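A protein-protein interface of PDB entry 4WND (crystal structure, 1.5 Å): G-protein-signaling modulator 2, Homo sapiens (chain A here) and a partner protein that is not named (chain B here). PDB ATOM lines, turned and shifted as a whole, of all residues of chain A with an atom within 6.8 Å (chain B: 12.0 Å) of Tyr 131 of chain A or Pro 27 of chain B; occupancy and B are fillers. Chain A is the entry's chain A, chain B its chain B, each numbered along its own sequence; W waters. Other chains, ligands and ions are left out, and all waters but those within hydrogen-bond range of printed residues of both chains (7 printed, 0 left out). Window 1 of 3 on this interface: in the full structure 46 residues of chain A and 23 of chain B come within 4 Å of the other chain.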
ATOM      1  N   ASN A  95      26.206 -11.410  -5.355  1.00  0.00           N
ATOM      2  CA  ASN A  95      25.071 -10.512  -5.467  1.00  0.00           C
ATOM      3  C   ASN A  95      24.320 -10.394  -4.152  1.00  0.00           C
ATOM      4  O   ASN A  95      23.752  -9.359  -3.851  1.00  0.00           O
ATOM      5  CB  ASN A  95      24.151 -10.965  -6.602  1.00  0.00           C
ATOM      6  CG  ASN A  95      24.703 -10.596  -7.977  1.00  0.00           C
ATOM      7  OD1 ASN A  95      25.757  -9.999  -8.080  1.00  0.00           O
ATOM      8  ND2 ASN A  95      23.983 -10.945  -9.042  1.00  0.00           N
ATOM      9  N   GLU A 126      30.473 -14.835 -18.467  1.00  0.00           N
ATOM     10  CA  GLU A 126      31.437 -13.740 -18.366  1.00  0.00           C
ATOM     11  C   GLU A 126      30.707 -12.382 -18.417  1.00  0.00           C
ATOM     12  O   GLU A 126      30.952 -11.509 -17.594  1.00  0.00           O
ATOM     13  CB  GLU A 126      32.451 -13.834 -19.517  1.00  0.00           C
ATOM     14  CG  GLU A 126      33.477 -12.727 -19.517  1.00  0.00           C
ATOM     15  CD  GLU A 126      34.476 -12.816 -20.686  1.00  0.00           C
ATOM     16  OE1 GLU A 126      34.338 -13.698 -21.566  1.00  0.00           O
ATOM     17  OE2 GLU A 126      35.413 -11.979 -20.696  1.00  0.00           O
ATOM     18  N   ALA A 127      29.828 -12.191 -19.408  1.00  0.00           N
ATOM     19  CA  ALA A 127      29.097 -10.952 -19.522  1.00  0.00           C
ATOM     20  C   ALA A 127      28.264 -10.676 -18.272  1.00  0.00           C
ATOM     21  O   ALA A 127      28.252  -9.560 -17.746  1.00  0.00           O
ATOM     22  CB  ALA A 127      28.216 -10.969 -20.765  1.00  0.00           C
ATOM     23  N   ARG A 128      27.567 -11.700 -17.784  1.00  0.00           N
ATOM     24  CA  ARG A 128      26.731 -11.505 -16.615  1.00  0.00           C
ATOM     25  C   ARG A 128      27.572 -11.127 -15.407  1.00  0.00           C
ATOM     26  O   ARG A 128      27.174 -10.254 -14.628  1.00  0.00           O
ATOM     27  CB  ARG A 128      25.896 -12.762 -16.343  1.00  0.00           C
ATOM     28  CG  ARG A 128      24.796 -12.925 -17.373  1.00  0.00           C
ATOM     29  CD  ARG A 128      24.203 -14.297 -17.397  1.00  0.00           C
ATOM     30  NE  ARG A 128      23.337 -14.493 -16.255  1.00  0.00           N
ATOM     31  CZ  ARG A 128      22.052 -14.136 -16.209  1.00  0.00           C
ATOM     32  NH1 ARG A 128      21.473 -13.543 -17.248  1.00  0.00           N
ATOM     33  NH2 ARG A 128      21.346 -14.358 -15.113  1.00  0.00           N
ATOM     34  N   ALA A 129      28.724 -11.762 -15.256  1.00  0.00           N
ATOM     35  CA  ALA A 129      29.617 -11.394 -14.146  1.00  0.00           C
ATOM     36  C   ALA A 129      30.115  -9.941 -14.236  1.00  0.00           C
ATOM     37  O   ALA A 129      30.250  -9.263 -13.225  1.00  0.00           O
ATOM     38  CB  ALA A 129      30.782 -12.351 -14.029  1.00  0.00           C
ATOM     39  N   LEU A 130      30.408  -9.490 -15.457  1.00  0.00           N
ATOM     40  CA  LEU A 130      30.854  -8.105 -15.654  1.00  0.00           C
ATOM     41  C   LEU A 130      29.784  -7.121 -15.250  1.00  0.00           C
ATOM     42  O   LEU A 130      30.072  -6.128 -14.572  1.00  0.00           O
ATOM     43  CB  LEU A 130      31.261  -7.873 -17.107  1.00  0.00           C
ATOM     44  CG  LEU A 130      32.527  -8.579 -17.550  1.00  0.00           C
ATOM     45  CD1 LEU A 130      32.621  -8.600 -19.069  1.00  0.00           C
ATOM     46  CD2 LEU A 130      33.755  -7.914 -16.948  1.00  0.00           C
ATOM     47  N   TYR A 131      28.529  -7.369 -15.662  1.00  0.00           N
ATOM     48  CA  TYR A 131      27.387  -6.566 -15.217  1.00  0.00           C
ATOM     49  C   TYR A 131      27.255  -6.566 -13.688  1.00  0.00           C
ATOM     50  O   TYR A 131      27.091  -5.516 -13.067  1.00  0.00           O
ATOM     51  CB  TYR A 131      26.101  -7.059 -15.860  1.00  0.00           C
ATOM     52  CG  TYR A 131      24.843  -6.287 -15.589  1.00  0.00           C
ATOM     53  CD1 TYR A 131      24.575  -5.085 -16.225  1.00  0.00           C
ATOM     54  CD2 TYR A 131      23.848  -6.805 -14.764  1.00  0.00           C
ATOM     55  CE1 TYR A 131      23.392  -4.405 -16.016  1.00  0.00           C
ATOM     56  CE2 TYR A 131      22.677  -6.142 -14.566  1.00  0.00           C
ATOM     57  CZ  TYR A 131      22.423  -4.955 -15.219  1.00  0.00           C
ATOM     58  OH  TYR A 131      21.222  -4.276 -15.081  1.00  0.00           O
ATOM     59  N   ASN A 132      27.370  -7.754 -13.078  1.00  0.00           N
ATOM     60  CA  ASN A 132      27.312  -7.817 -11.648  1.00  0.00           C
ATOM     61  C   ASN A 132      28.408  -7.001 -10.952  1.00  0.00           C
ATOM     62  O   ASN A 132      28.136  -6.341  -9.963  1.00  0.00           O
ATOM     63  CB  ASN A 132      27.426  -9.278 -11.166  1.00  0.00           C
ATOM     64  CG  ASN A 132      26.220 -10.106 -11.507  1.00  0.00           C
ATOM     65  OD1 ASN A 132      25.147  -9.609 -11.716  1.00  0.00           O
ATOM     66  ND2 ASN A 132      26.410 -11.411 -11.512  1.00  0.00           N
ATOM     67  N   LEU A 133      29.624  -7.063 -11.472  1.00  0.00           N
ATOM     68  CA  LEU A 133      30.746  -6.276 -10.923  1.00  0.00           C
ATOM     69  C   LEU A 133      30.513  -4.780 -11.080  1.00  0.00           C
ATOM     70  O   LEU A 133      30.726  -4.010 -10.132  1.00  0.00           O
ATOM     71  CB  LEU A 133      32.072  -6.693 -11.547  1.00  0.00           C
ATOM     72  CG  LEU A 133      32.602  -8.014 -10.961  1.00  0.00           C
ATOM     73  CD1 LEU A 133      33.565  -8.692 -11.908  1.00  0.00           C
ATOM     74  CD2 LEU A 133      33.291  -7.761  -9.621  1.00  0.00           C
ATOM     75  N   GLY A 134      29.939  -4.355 -12.204  1.00  0.00           N
ATOM     76  CA  GLY A 134      29.573  -2.970 -12.324  1.00  0.00           C
ATOM     77  C   GLY A 134      28.568  -2.569 -11.247  1.00  0.00           C
ATOM     78  O   GLY A 134      28.677  -1.514 -10.618  1.00  0.00           O
ATOM     79  N   ASN A 135      27.554  -3.414 -11.035  1.00  0.00           N
ATOM     80  CA  ASN A 135      26.561  -3.149 -10.028  1.00  0.00           C
ATOM     81  C   ASN A 135      27.133  -3.098  -8.613  1.00  0.00           C
ATOM     82  O   ASN A 135      26.734  -2.235  -7.827  1.00  0.00           O
ATOM     83  CB  ASN A 135      25.441  -4.173 -10.077  1.00  0.00           C
ATOM     84  CG  ASN A 135      24.639  -4.123 -11.358  1.00  0.00           C
ATOM     85  OD1 ASN A 135      24.617  -3.128 -12.095  1.00  0.00           O
ATOM     86  ND2 ASN A 135      23.907  -5.204 -11.607  1.00  0.00           N
ATOM     87  N   VAL A 136      28.051  -3.994  -8.295  1.00  0.00           N
ATOM     88  CA  VAL A 136      28.685  -3.940  -6.963  1.00  0.00           C
ATOM     89  C   VAL A 136      29.436  -2.610  -6.774  1.00  0.00           C
ATOM     90  O   VAL A 136      29.298  -1.951  -5.727  1.00  0.00           O
ATOM     91  CB  VAL A 136      29.651  -5.109  -6.735  1.00  0.00           C
ATOM     92  CG1 VAL A 136      30.293  -4.937  -5.369  1.00  0.00           C
ATOM     93  CG2 VAL A 136      28.950  -6.429  -6.772  1.00  0.00           C
ATOM     94  N   PHE A 169      33.495  -1.601 -15.787  1.00  0.00           N
ATOM     95  CA  PHE A 169      32.818  -2.907 -15.885  1.00  0.00           C
ATOM     96  C   PHE A 169      31.607  -2.853 -16.784  1.00  0.00           C
ATOM     97  O   PHE A 169      31.405  -3.799 -17.572  1.00  0.00           O
ATOM     98  CB  PHE A 169      32.453  -3.477 -14.519  1.00  0.00           C
ATOM     99  CG  PHE A 169      33.604  -4.135 -13.825  1.00  0.00           C
ATOM    100  CD1 PHE A 169      34.145  -5.316 -14.313  1.00  0.00           C
ATOM    101  CD2 PHE A 169      34.140  -3.587 -12.674  1.00  0.00           C
ATOM    102  CE1 PHE A 169      35.222  -5.940 -13.670  1.00  0.00           C
ATOM    103  CE2 PHE A 169      35.203  -4.212 -12.009  1.00  0.00           C
ATOM    104  CZ  PHE A 169      35.745  -5.385 -12.512  1.00  0.00           C
ATOM    105  N   TYR A 170      30.814  -1.788 -16.710  1.00  0.00           N
ATOM    106  CA  TYR A 170      29.663  -1.682 -17.587  1.00  0.00           C
ATOM    107  C   TYR A 170      30.090  -1.582 -19.053  1.00  0.00           C
ATOM    108  O   TYR A 170      29.469  -2.174 -19.924  1.00  0.00           O
ATOM    109  CB  TYR A 170      28.762  -0.535 -17.216  1.00  0.00           C
ATOM    110  CG  TYR A 170      28.024  -0.649 -15.897  1.00  0.00           C
ATOM    111  CD1 TYR A 170      27.341  -1.825 -15.544  1.00  0.00           C
ATOM    112  CD2 TYR A 170      27.958   0.426 -15.009  1.00  0.00           C
ATOM    113  CE1 TYR A 170      26.641  -1.909 -14.369  1.00  0.00           C
ATOM    114  CE2 TYR A 170      27.236   0.344 -13.829  1.00  0.00           C
ATOM    115  CZ  TYR A 170      26.595  -0.836 -13.502  1.00  0.00           C
ATOM    116  OH  TYR A 170      25.884  -0.861 -12.346  1.00  0.00           O
ATOM    117  N   ASN A 173      31.133  -5.020 -20.104  1.00  0.00           N
ATOM    118  CA  ASN A 173      29.906  -5.777 -20.345  1.00  0.00           C
ATOM    119  C   ASN A 173      29.266  -5.420 -21.688  1.00  0.00           C
ATOM    120  O   ASN A 173      28.895  -6.296 -22.462  1.00  0.00           O
ATOM    121  CB  ASN A 173      28.889  -5.564 -19.199  1.00  0.00           C
ATOM    122  CG  ASN A 173      27.536  -6.152 -19.511  1.00  0.00           C
ATOM    123  OD1 ASN A 173      26.615  -5.440 -19.881  1.00  0.00           O
ATOM    124  ND2 ASN A 173      27.411  -7.456 -19.356  1.00  0.00           N
ATOM    125  N   ALA A 185      20.249  -7.012 -23.277  1.00  0.00           N
ATOM    126  CA  ALA A 185      21.350  -6.855 -22.295  1.00  0.00           C
ATOM    127  C   ALA A 185      22.132  -5.556 -22.569  1.00  0.00           C
ATOM    128  O   ALA A 185      22.557  -4.875 -21.608  1.00  0.00           O
ATOM    129  CB  ALA A 185      22.279  -8.015 -22.324  1.00  0.00           C
ATOM    130  N   ARG A 188      20.252  -2.778 -20.853  1.00  0.00           N
ATOM    131  CA  ARG A 188      20.409  -2.745 -19.413  1.00  0.00           C
ATOM    132  C   ARG A 188      21.764  -2.126 -19.051  1.00  0.00           C
ATOM    133  O   ARG A 188      21.860  -1.368 -18.119  1.00  0.00           O
ATOM    134  CB  ARG A 188      20.264  -4.095 -18.823  1.00  0.00           C
ATOM    135  CG  ARG A 188      18.818  -4.606 -18.887  1.00  0.00           C
ATOM    136  CD  ARG A 188      18.686  -5.910 -18.130  1.00  0.00           C
ATOM    137  NE  ARG A 188      19.354  -7.048 -18.754  1.00  0.00           N
ATOM    138  CZ  ARG A 188      18.849  -7.815 -19.746  1.00  0.00           C
ATOM    139  NH1 ARG A 188      19.547  -8.839 -20.183  1.00  0.00           N
ATOM    140  NH2 ARG A 188      17.686  -7.527 -20.345  1.00  0.00           N
ATOM    141  N   ALA A 189      22.792  -2.518 -19.772  1.00  0.00           N
ATOM    142  CA  ALA A 189      24.129  -1.911 -19.554  1.00  0.00           C
ATOM    143  C   ALA A 189      24.065  -0.418 -19.742  1.00  0.00           C
ATOM    144  O   ALA A 189      24.636   0.350 -18.940  1.00  0.00           O
ATOM    145  CB  ALA A 189      25.131  -2.504 -20.519  1.00  0.00           C
ATOM    146  N   PHE A 190      23.427   0.038 -20.806  1.00  0.00           N
ATOM    147  CA  PHE A 190      23.366   1.463 -21.063  1.00  0.00           C
ATOM    148  C   PHE A 190      22.678   2.214 -19.910  1.00  0.00           C
ATOM    149  O   PHE A 190      23.088   3.311 -19.553  1.00  0.00           O
ATOM    150  CB  PHE A 190      22.627   1.793 -22.351  1.00  0.00           C
ATOM    151  CG  PHE A 190      23.459   1.673 -23.608  1.00  0.00           C
ATOM    152  CD1 PHE A 190      24.563   2.503 -23.815  1.00  0.00           C
ATOM    153  CD2 PHE A 190      23.094   0.791 -24.612  1.00  0.00           C
ATOM    154  CE1 PHE A 190      25.296   2.417 -24.993  1.00  0.00           C
ATOM    155  CE2 PHE A 190      23.852   0.676 -25.762  1.00  0.00           C
ATOM    156  CZ  PHE A 190      24.935   1.511 -25.958  1.00  0.00           C
ATOM    157  N   ASN A 192      22.419   1.481 -16.615  1.00  0.00           N
ATOM    158  CA  ASN A 192      23.220   1.543 -15.401  1.00  0.00           C
ATOM    159  C   ASN A 192      24.477   2.362 -15.648  1.00  0.00           C
ATOM    160  O   ASN A 192      24.906   3.098 -14.775  1.00  0.00           O
ATOM    161  CB  ASN A 192      23.559   0.161 -14.894  1.00  0.00           C
ATOM    162  CG  ASN A 192      22.404  -0.477 -14.143  1.00  0.00           C
ATOM    163  OD1 ASN A 192      21.340   0.117 -14.032  1.00  0.00           O
ATOM    164  ND2 ASN A 192      22.602  -1.696 -13.642  1.00  0.00           N
ATOM    165  N   ARG A 213      19.538   3.560 -24.236  1.00  0.00           N
ATOM    166  CA  ARG A 213      18.650   2.786 -23.422  1.00  0.00           C
ATOM    167  C   ARG A 213      17.188   2.939 -23.945  1.00  0.00           C
ATOM    168  O   ARG A 213      16.454   1.948 -24.059  1.00  0.00           O
ATOM    169  CB  ARG A 213      18.741   3.255 -21.974  1.00  0.00           C
ATOM    170  CG  ARG A 213      18.374   2.189 -20.993  1.00  0.00           C
ATOM    171  CD  ARG A 213      16.848   1.915 -20.805  1.00  0.00           C
ATOM    172  NE  ARG A 213      16.675   0.589 -20.260  1.00  0.00           N
ATOM    173  CZ  ARG A 213      16.640  -0.538 -21.004  1.00  0.00           C
ATOM    174  NH1 ARG A 213      16.632  -0.471 -22.340  1.00  0.00           N
ATOM    175  NH2 ARG A 213      16.623  -1.698 -20.401  1.00  0.00           N
ATOM    176  N   ASP A 222       9.343  -2.345 -24.515  1.00  0.00           N
ATOM    177  CA  ASP A 222       9.483  -2.563 -23.088  1.00  0.00           C
ATOM    178  C   ASP A 222       9.079  -1.259 -22.412  1.00  0.00           C
ATOM    179  O   ASP A 222       9.835  -0.276 -22.428  1.00  0.00           O
ATOM    180  CB  ASP A 222      10.938  -2.955 -22.736  1.00  0.00           C
ATOM    181  CG  ASP A 222      11.146  -3.231 -21.252  1.00  0.00           C
ATOM    182  OD1 ASP A 222      10.312  -2.820 -20.374  1.00  0.00           O
ATOM    183  OD2 ASP A 222      12.176  -3.852 -20.909  1.00  0.00           O
ATOM    184  N   ARG A 228      11.811   4.244 -17.462  1.00  0.00           N
ATOM    185  CA  ARG A 228      13.055   4.477 -16.742  1.00  0.00           C
ATOM    186  C   ARG A 228      13.947   5.433 -17.515  1.00  0.00           C
ATOM    187  O   ARG A 228      14.512   6.389 -16.933  1.00  0.00           O
ATOM    188  CB  ARG A 228      13.805   3.167 -16.490  1.00  0.00           C
ATOM    189  CG  ARG A 228      13.143   2.242 -15.507  1.00  0.00           C
ATOM    190  CD  ARG A 228      14.083   1.149 -15.036  1.00  0.00           C
ATOM    191  NE  ARG A 228      14.474   0.223 -16.087  1.00  0.00           N
ATOM    192  CZ  ARG A 228      13.787  -0.871 -16.442  1.00  0.00           C
ATOM    193  NH1 ARG A 228      12.593  -1.136 -15.907  1.00  0.00           N
ATOM    194  NH2 ARG A 228      14.259  -1.678 -17.359  1.00  0.00           N
ATOM    195  N   MET B  23      16.798   7.671  -8.795  1.00  0.00           N
ATOM    196  CA  MET B  23      16.970   7.310 -10.171  1.00  0.00           C
ATOM    197  C   MET B  23      16.640   5.843 -10.395  1.00  0.00           C
ATOM    198  O   MET B  23      16.596   5.042  -9.469  1.00  0.00           O
ATOM    199  CB  MET B  23      18.361   7.641 -10.674  1.00  0.00           C
ATOM    200  CG  MET B  23      19.472   6.937  -9.959  1.00  0.00           C
ATOM    201  SD  MET B  23      21.085   7.672 -10.335  1.00  0.00           S
ATOM    202  CE  MET B  23      22.113   6.462  -9.501  1.00  0.00           C
ATOM    203  N   GLU B  24      16.426   5.519 -11.653  1.00  0.00           N
ATOM    204  CA  GLU B  24      15.810   4.262 -12.024  1.00  0.00           C
ATOM    205  C   GLU B  24      16.916   3.343 -12.564  1.00  0.00           C
ATOM    206  O   GLU B  24      17.318   3.485 -13.720  1.00  0.00           O
ATOM    207  CB  GLU B  24      14.735   4.514 -13.091  1.00  0.00           C
ATOM    208  CG  GLU B  24      13.430   5.157 -12.567  1.00  0.00           C
ATOM    209  CD  GLU B  24      12.427   4.121 -12.063  1.00  0.00           C
ATOM    210  OE1 GLU B  24      12.741   2.907 -12.045  1.00  0.00           O
ATOM    211  OE2 GLU B  24      11.313   4.514 -11.695  1.00  0.00           O
ATOM    212  N   MET B  25      17.377   2.402 -11.730  1.00  0.00           N
ATOM    213  CA  MET B  25      18.394   1.425 -12.149  1.00  0.00           C
ATOM    214  C   MET B  25      17.760   0.230 -12.836  1.00  0.00           C
ATOM    215  O   MET B  25      16.554   0.034 -12.790  1.00  0.00           O
ATOM    216  CB  MET B  25      19.233   0.936 -10.968  1.00  0.00           C
ATOM    217  CG  MET B  25      19.965   2.047 -10.203  1.00  0.00           C
ATOM    218  SD  MET B  25      21.170   2.988 -11.189  1.00  0.00           S
ATOM    219  CE  MET B  25      22.499   1.821 -11.346  1.00  0.00           C
ATOM    220  N   GLU B  26      18.584  -0.535 -13.537  1.00  0.00           N
ATOM    221  CA  GLU B  26      18.095  -1.614 -14.410  1.00  0.00           C
ATOM    222  C   GLU B  26      17.938  -2.889 -13.601  1.00  0.00           C
ATOM    223  O   GLU B  26      18.443  -2.980 -12.490  1.00  0.00           O
ATOM    224  CB  GLU B  26      19.049  -1.808 -15.594  1.00  0.00           C
ATOM    225  CG  GLU B  26      18.964  -0.652 -16.575  1.00  0.00           C
ATOM    226  CD  GLU B  26      17.618  -0.588 -17.265  1.00  0.00           C
ATOM    227  OE1 GLU B  26      17.080   0.560 -17.447  1.00  0.00           O
ATOM    228  OE2 GLU B  26      17.142  -1.652 -17.699  1.00  0.00           O
ATOM    229  N   PRO B  27      17.215  -3.873 -14.165  1.00  0.00           N
ATOM    230  CA  PRO B  27      17.025  -5.099 -13.428  1.00  0.00           C
ATOM    231  C   PRO B  27      18.326  -5.786 -13.128  1.00  0.00           C
ATOM    232  O   PRO B  27      19.262  -5.767 -13.972  1.00  0.00           O
ATOM    233  CB  PRO B  27      16.184  -5.956 -14.360  1.00  0.00           C
ATOM    234  CG  PRO B  27      15.471  -5.001 -15.203  1.00  0.00           C
ATOM    235  CD  PRO B  27      16.354  -3.797 -15.349  1.00  0.00           C
ATOM    236  N   GLU B  28      18.341  -6.433 -11.980  1.00  0.00           N
ATOM    237  CA  GLU B  28      19.471  -7.227 -11.507  1.00  0.00           C
ATOM    238  C   GLU B  28      19.190  -8.684 -11.784  1.00  0.00           C
ATOM    239  O   GLU B  28      18.043  -9.082 -12.045  1.00  0.00           O
ATOM    240  CB  GLU B  28      19.710  -6.994 -10.027  1.00  0.00           C
ATOM    241  CG  GLU B  28      20.262  -5.601  -9.703  1.00  0.00           C
ATOM    242  CD  GLU B  28      20.121  -5.209  -8.233  1.00  0.00           C
ATOM    243  OE1 GLU B  28      19.472  -5.943  -7.450  1.00  0.00           O
ATOM    244  OE2 GLU B  28      20.638  -4.131  -7.868  1.00  0.00           O
ATOM    245  N   THR B  29      20.262  -9.477 -11.797  1.00  0.00           N
ATOM    246  CA  THR B  29      20.171 -10.858 -12.147  1.00  0.00           C
ATOM    247  C   THR B  29      20.568 -11.717 -10.961  1.00  0.00           C
ATOM    248  O   THR B  29      21.235 -11.263 -10.014  1.00  0.00           O
ATOM    249  CB  THR B  29      21.153 -11.222 -13.315  1.00  0.00           C
ATOM    250  OG1 THR B  29      22.509 -10.934 -12.934  1.00  0.00           O
ATOM    251  CG2 THR B  29      20.804 -10.410 -14.586  1.00  0.00           C
ATOM    252  N   MET B  30      20.139 -12.951 -11.017  1.00  0.00           N
ATOM    253  CA  MET B  30      20.828 -14.039 -10.305  1.00  0.00           C
ATOM    254  C   MET B  30      21.122 -15.154 -11.297  1.00  0.00           C
ATOM    255  O   MET B  30      20.561 -15.201 -12.397  1.00  0.00           O
ATOM    256  CB  MET B  30      20.020 -14.541  -9.121  1.00  0.00           C
ATOM    257  CG  MET B  30      19.707 -13.474  -8.087  1.00  0.00           C
ATOM    258  SD  MET B  30      21.182 -12.878  -7.207  1.00  0.00           S
ATOM    259  CE  MET B  30      21.261 -14.047  -5.889  1.00  0.00           C
ATOM    260  N   GLU B  31      22.048 -16.047 -10.926  1.00  0.00           N
ATOM    261  CA  GLU B  31      22.323 -17.233 -11.701  1.00  0.00           C
ATOM    262  C   GLU B  31      21.380 -18.360 -11.282  1.00  0.00           C
ATOM    263  O   GLU B  31      21.087 -18.535 -10.109  1.00  0.00           O
ATOM    264  CB  GLU B  31      23.776 -17.693 -11.522  1.00  0.00           C
ATOM    265  CG  GLU B  31      24.787 -16.688 -12.001  1.00  0.00           C
ATOM    266  CD  GLU B  31      24.561 -16.349 -13.446  1.00  0.00           C
ATOM    267  OE1 GLU B  31      24.417 -15.126 -13.767  1.00  0.00           O
ATOM    268  OE2 GLU B  31      24.500 -17.273 -14.295  1.00  0.00           O
HETATM  269  O   HOH W   1      23.890 -13.067 -12.044  1.00  0.00           O
HETATM  270  O   HOH W   2      21.098  -3.140 -11.785  1.00  0.00           O
HETATM  271  O   HOH W   3      22.839  -8.127 -11.378  1.00  0.00           O
HETATM  272  O   HOH W   4      24.426 -13.986  -9.533  1.00  0.00           O
HETATM  273  O   HOH W   5      25.019 -17.392 -17.070  1.00  0.00           O
HETATM  274  O   HOH W   6      19.364 -16.672 -14.435  1.00  0.00           O
HETATM  275  O   HOH W   7      24.249 -10.237 -14.805  1.00  0.00           O
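Pro 27 of chain B touches just these residues of chain A: Tyr 131 (2.7 Å) and Arg 228 (3.6 Å). No residue of chain B comes within 4 Å of Ala 127 of chain A. No residue of chain B comes within 4 Å of Leu 130 of chain A. Of chain B, only Thr 29 (3.2 Å) comes within 4 Å of Asn 132 of chain A. No residue of chain B comes within 4 Å of Leu 133 of chain A. Gly 134 of chain A touches none of the printed residues of chain B. Asn 135 of chain A touches none of the printed residues of chain B. Arg 188 of chain A touches just one residue of chain B: Glu 26. No residue of chain B comes within 4 Å of Ala 189 of chain A. Asn 192 of chain A touches just these residues of chain B: Met 25 (3.4 Å) and Glu 26 (2.9 Å). Of the printed residues of chain A, Glu 24 of chain B touches Arg 228 (3.5 Å). Printed residues of chain B within 4 Å of Arg 213 of chain A: Glu 26 (2.8 Å). Of the printed residues of chain A, Met 30 of chain B touches Asn 95 (3.6 Å) and Arg 128 (3.0 Å). Printed residues of chain B within 4 Å of Arg 228 of chain A: Glu 24 (3.5 Å), Met 25 (3.5 Å), Glu 26 (2.9 Å) and Pro 27 (3.6 Å). Of the printed residues of chain A, Glu 31 of chain B touches Arg 128 (2.8 Å). Phe 169 of chain A touches none of the printed residues of chain B. The nearest residue of chain A that does not touch Pro 27 of chain B is Arg 188 of chain A (4.2 Å). The nearest printed residue of chain A that does not touch Thr 29 of chain B is Tyr 131 of chain A (4.7 Å).
The backbone carbonyl oxygen (O) of Arg 128 of chain A sits close to the side-chain amide nitrogen (ND2) of Asn 132 of chain A. OD1 of Asn 135 of chain A is in hydrogen-bond range of ND2 of Asn 192 of chain A, 2.9 Å away. The side-chain hydroxyl of Tyr 131 of chain A lies within hydrogen-bond range of the side-chain amide nitrogen of Asn 192 of chain A (3.3 Å). The side-chain amide oxygen of Asn 132 of chain A sits at hydrogen-bond distance from the side-chain amide nitrogen of Asn 95 of chain A, 3.2 Å away.
OD1 of Asn 132 of chain A is in hydrogen-bond range of OG1 of Thr 29 of chain B, at 3.2 Å. NH2 of Arg 213 of chain A lies within salt-bridge range of OE2 of Glu 26 of chain B, at 2.8 Å. OD1 of Asn 192 of chain A lies within hydrogen-bond range of N of Glu 26 of chain B, at 2.9 Å. The backbone carbonyl oxygen (O) of Thr 29 of chain B sits at hydrogen-bond distance from the side-chain amide nitrogen (ND2) of Asn 95 of chain A (2.9 Å). The side-chain carboxylate of Glu 26 of chain B is in salt-bridge range of the guanidinium group of Arg 228 of chain A (2.9 Å). The guanidinium group (NH2) of Arg 128 of chain A lies within hydrogen-bond range of the backbone carbonyl oxygen (O) of Met 30 of chain B (3.0 Å). The side-chain hydroxyl (OH) of Tyr 131 of chain A lies within hydrogen-bond range of the backbone carbonyl oxygen (O) of Pro 27 of chain B, at 2.7 Å. OE1 of Glu 31 of chain B lies within salt-bridge range of NE of Arg 128 of chain A, at 2.8 Å.
Printed residues of chain A that touch a printed residue of chain B: Asn 95, Arg 128, Tyr 131, Asn 132, Arg 188, Asn 192, Arg 213 and Arg 228. Hydrophobic or aromatic side chains of chain A that line the printed part of chain B: Tyr 131. Of the 9 printed residues of chain B, 7 touch a printed residue of chain A. Among the printed residues, 16 pairs touch across the chains. Among the printed residues, Asp or Glu carboxylates within 4 Å of a Lys or Arg side-chain nitrogen of the other chain: Arg 128 of chain A with Glu 31 of chain B, Arg 213 of chain A with Glu 26 of chain B and Arg 228 of chain A with Glu 26 of chain B.
Water W7 lies within hydrogen-bond range of the side-chain hydroxyl (OG1) of Thr 29 of chain B (2.6 Å), the backbone carbonyl oxygen (O) of Arg 128 of chain A (2.9 Å) and the side-chain amide oxygen (OD1) of Asn 132 of chain A (3.3 Å). Water W1 lies within hydrogen-bond range of OG1 of Thr 29 of chain B (2.7 Å), OE1 of Glu 31 of chain B (2.7 Å) and ND2 of Asn 132 of chain A (3.1 Å). Water W2 lies within hydrogen-bond range of O of Glu 26 of chain B (2.8 Å), ND2 of Asn 192 of chain A (2.8 Å), OH of Tyr 131 of chain A (3.5 Å) and ND2 of Asn 135 of chain A (3.5 Å). Water W3 lies within hydrogen-bond range of OD1 of Asn 132 of chain A (2.8 Å), N of Thr 29 of chain B (2.9 Å) and ND2 of Asn 135 of chain A (3.1 Å). Water W5 bridges the side-chain carboxylate of Glu 31 of chain B and the guanidinium group of Arg 128 of chain A. Water W4 lies within hydrogen-bond range of the side-chain amide nitrogen (ND2) of Asn 95 of chain A (3.1 Å) and the backbone NH (N) of Glu 31 of chain B (3.4 Å).
Met 30 of chain B touches Asn 95 of chain A. Arg 128 of chain A touches Thr 29 of chain B. OH of Tyr 131 of chain A touches CB of Glu 26 of chain B, 3.3 Å away. Arg 188 of chain A touches Glu 26 of chain B. Asn 192 of chain A touches Met 25 of chain B. Glu 24 of chain B touches Arg 228 of chain A. Met 25 of chain B touches Arg 228 of chain A. Arg 228 of chain A touches Pro 27 of chain B.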
